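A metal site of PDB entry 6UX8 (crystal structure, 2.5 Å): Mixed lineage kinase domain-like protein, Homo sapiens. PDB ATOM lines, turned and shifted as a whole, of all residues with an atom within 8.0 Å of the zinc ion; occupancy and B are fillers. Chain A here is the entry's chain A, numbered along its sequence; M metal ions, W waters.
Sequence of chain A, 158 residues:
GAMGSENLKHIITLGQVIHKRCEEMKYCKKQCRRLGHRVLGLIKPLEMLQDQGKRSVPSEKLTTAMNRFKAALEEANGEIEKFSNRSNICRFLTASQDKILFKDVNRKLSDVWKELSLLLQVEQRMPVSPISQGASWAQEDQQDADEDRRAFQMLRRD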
ATOM      1  N   HIS A  19       9.133  19.438   1.390  1.00  0.00           N
ATOM      2  CA  HIS A  19       8.365  20.376   0.581  1.00  0.00           C
ATOM      3  C   HIS A  19       6.889  19.993   0.508  1.00  0.00           C
ATOM      4  O   HIS A  19       6.019  20.858   0.517  1.00  0.00           O
ATOM      5  CB  HIS A  19       8.967  20.467  -0.829  1.00  0.00           C
ATOM      6  CG  HIS A  19       8.131  21.255  -1.787  1.00  0.00           C
ATOM      7  ND1 HIS A  19       7.504  20.674  -2.876  1.00  0.00           N
ATOM      8  CD2 HIS A  19       7.797  22.559  -1.816  1.00  0.00           C
ATOM      9  CE1 HIS A  19       6.838  21.601  -3.541  1.00  0.00           C
ATOM     10  NE2 HIS A  19       6.996  22.753  -2.915  1.00  0.00           N
ATOM     11  N   LYS A  20       6.601  18.694   0.435  1.00  0.00           N
ATOM     12  CA  LYS A  20       5.219  18.248   0.361  1.00  0.00           C
ATOM     13  C   LYS A  20       4.481  18.525   1.668  1.00  0.00           C
ATOM     14  O   LYS A  20       3.293  18.862   1.659  1.00  0.00           O
ATOM     15  CB  LYS A  20       5.155  16.766   0.022  1.00  0.00           C
ATOM     16  N   CYS A  22       5.176  21.013   3.761  1.00  0.00           N
ATOM     17  CA  CYS A  22       4.978  22.462   3.886  1.00  0.00           C
ATOM     18  C   CYS A  22       3.742  22.910   3.129  1.00  0.00           C
ATOM     19  O   CYS A  22       3.031  23.829   3.578  1.00  0.00           O
ATOM     20  CB  CYS A  22       6.215  23.203   3.387  1.00  0.00           C
ATOM     21  SG  CYS A  22       7.671  23.034   4.448  1.00  0.00           S
ATOM     22  N   GLU A  23       3.449  22.291   1.980  1.00  0.00           N
ATOM     23  CA  GLU A  23       2.255  22.636   1.225  1.00  0.00           C
ATOM     24  C   GLU A  23       0.987  22.232   1.959  1.00  0.00           C
ATOM     25  O   GLU A  23      -0.071  22.823   1.723  1.00  0.00           O
ATOM     26  CB  GLU A  23       2.293  21.976  -0.148  1.00  0.00           C
ATOM     27  CG  GLU A  23       3.533  22.279  -0.978  1.00  0.00           C
ATOM     28  CD  GLU A  23       3.522  23.678  -1.562  1.00  0.00           C
ATOM     29  OE1 GLU A  23       4.608  24.149  -1.995  1.00  0.00           O
ATOM     30  OE2 GLU A  23       2.445  24.305  -1.611  1.00  0.00           O
ATOM     31  N   CYS A  32       5.856  28.580   5.663  1.00  0.00           N
ATOM     32  CA  CYS A  32       6.005  27.157   5.372  1.00  0.00           C
ATOM     33  C   CYS A  32       6.371  26.936   3.902  1.00  0.00           C
ATOM     34  O   CYS A  32       7.320  26.203   3.598  1.00  0.00           O
ATOM     35  CB  CYS A  32       4.727  26.401   5.725  1.00  0.00           C
ATOM     36  SG  CYS A  32       4.247  26.542   7.457  1.00  0.00           S
ATOM     37  N   ARG A  33       5.627  27.565   2.988  1.00  0.00           N
ATOM     38  CA  ARG A  33       5.946  27.414   1.576  1.00  0.00           C
ATOM     39  C   ARG A  33       7.290  28.042   1.225  1.00  0.00           C
ATOM     40  O   ARG A  33       7.933  27.634   0.246  1.00  0.00           O
ATOM     41  CB  ARG A  33       4.832  28.019   0.722  1.00  0.00           C
ATOM     42  CG  ARG A  33       3.452  27.448   0.998  1.00  0.00           C
ATOM     43  CD  ARG A  33       2.395  28.025   0.079  1.00  0.00           C
ATOM     44  NE  ARG A  33       2.404  27.389  -1.240  1.00  0.00           N
ATOM     45  CZ  ARG A  33       3.018  27.874  -2.310  1.00  0.00           C
ATOM     46  NH1 ARG A  33       3.694  29.015  -2.238  1.00  0.00           N
ATOM     47  NH2 ARG A  33       2.975  27.216  -3.467  1.00  0.00           N
ATOM     48  N   ARG A  34       7.733  29.021   2.022  1.00  0.00           N
ATOM     49  CA  ARG A  34       9.066  29.579   1.831  1.00  0.00           C
ATOM     50  C   ARG A  34      10.145  28.565   2.214  1.00  0.00           C
ATOM     51  O   ARG A  34      11.163  28.455   1.525  1.00  0.00           O
ATOM     52  CB  ARG A  34       9.225  30.859   2.653  1.00  0.00           C
ATOM     53  CG  ARG A  34      10.588  31.524   2.535  1.00  0.00           C
ATOM     54  CD  ARG A  34      10.709  32.313   1.244  1.00  0.00           C
ATOM     55  NE  ARG A  34       9.781  33.440   1.222  1.00  0.00           N
ATOM     56  CZ  ARG A  34       9.718  34.327   0.238  1.00  0.00           C
ATOM     57  NH1 ARG A  34      10.528  34.221  -0.816  1.00  0.00           N
ATOM     58  NH2 ARG A  34       8.842  35.322   0.292  1.00  0.00           N
ATOM     59  N   GLY A  36       9.840  25.122   2.351  1.00  0.00           N
ATOM     60  CA  GLY A  36       9.842  23.991   1.442  1.00  0.00           C
ATOM     61  C   GLY A  36      10.444  24.301   0.089  1.00  0.00           C
ATOM     62  O   GLY A  36      11.072  23.438  -0.532  1.00  0.00           O
ATOM     63  N   HIS A  37      10.270  25.539  -0.390  1.00  0.00           N
ATOM     64  CA  HIS A  37      10.840  25.920  -1.671  1.00  0.00           C
ATOM     65  C   HIS A  37      12.334  26.205  -1.568  1.00  0.00           C
ATOM     66  O   HIS A  37      13.066  26.022  -2.550  1.00  0.00           O
ATOM     67  CB  HIS A  37      10.100  27.140  -2.239  1.00  0.00           C
ATOM     68  CG  HIS A  37       8.699  26.833  -2.666  1.00  0.00           C
ATOM     69  ND1 HIS A  37       7.731  27.808  -2.801  1.00  0.00           N
ATOM     70  CD2 HIS A  37       8.106  25.662  -3.002  1.00  0.00           C
ATOM     71  CE1 HIS A  37       6.605  27.254  -3.191  1.00  0.00           C
ATOM     72  NE2 HIS A  37       6.801  25.945  -3.318  1.00  0.00           N
ATOM     73  N   LEU A  40      13.838  22.805  -1.801  1.00  0.00           N
ATOM     74  CA  LEU A  40      13.868  22.371  -3.191  1.00  0.00           C
ATOM     75  C   LEU A  40      15.061  22.969  -3.931  1.00  0.00           C
ATOM     76  O   LEU A  40      15.680  22.310  -4.775  1.00  0.00           O
ATOM     77  CB  LEU A  40      12.565  22.736  -3.901  1.00  0.00           C
ATOM     78  CG  LEU A  40      11.310  21.964  -3.512  1.00  0.00           C
ATOM     79  CD1 LEU A  40      10.148  22.396  -4.383  1.00  0.00           C
ATOM     80  CD2 LEU A  40      11.545  20.470  -3.626  1.00  0.00           C
HETATM   81 ZN    ZN M   1       5.767  24.219  -3.613  1.00  0.00          ZN
HETATM   82  O   HOH W   1       4.454  23.724  -5.161  1.00  0.00           O
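The side-chain carboxylate (OE1) of Glu 23 is bound to the zinc ion.
NE2 of His 37 binds the zinc ion (2.0 Å).
A ring nitrogen (NE2) of His 19 binds the zinc ion (2.0 Å).
Water W1 binds the zinc ion.
The zinc ion has four donor atoms within binding distance.
The nearest printed residue that does not touch the zinc ion is Arg 33 (4.1 Å).
OE2 of Glu 23 lies within salt-bridge range of NE of Arg 33 (3.1 Å).
The backbone carbonyl oxygen (O) of Arg 33 is in hydrogen-bond range of a ring nitrogen (ND1) of His 37, at 3.1 Å.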
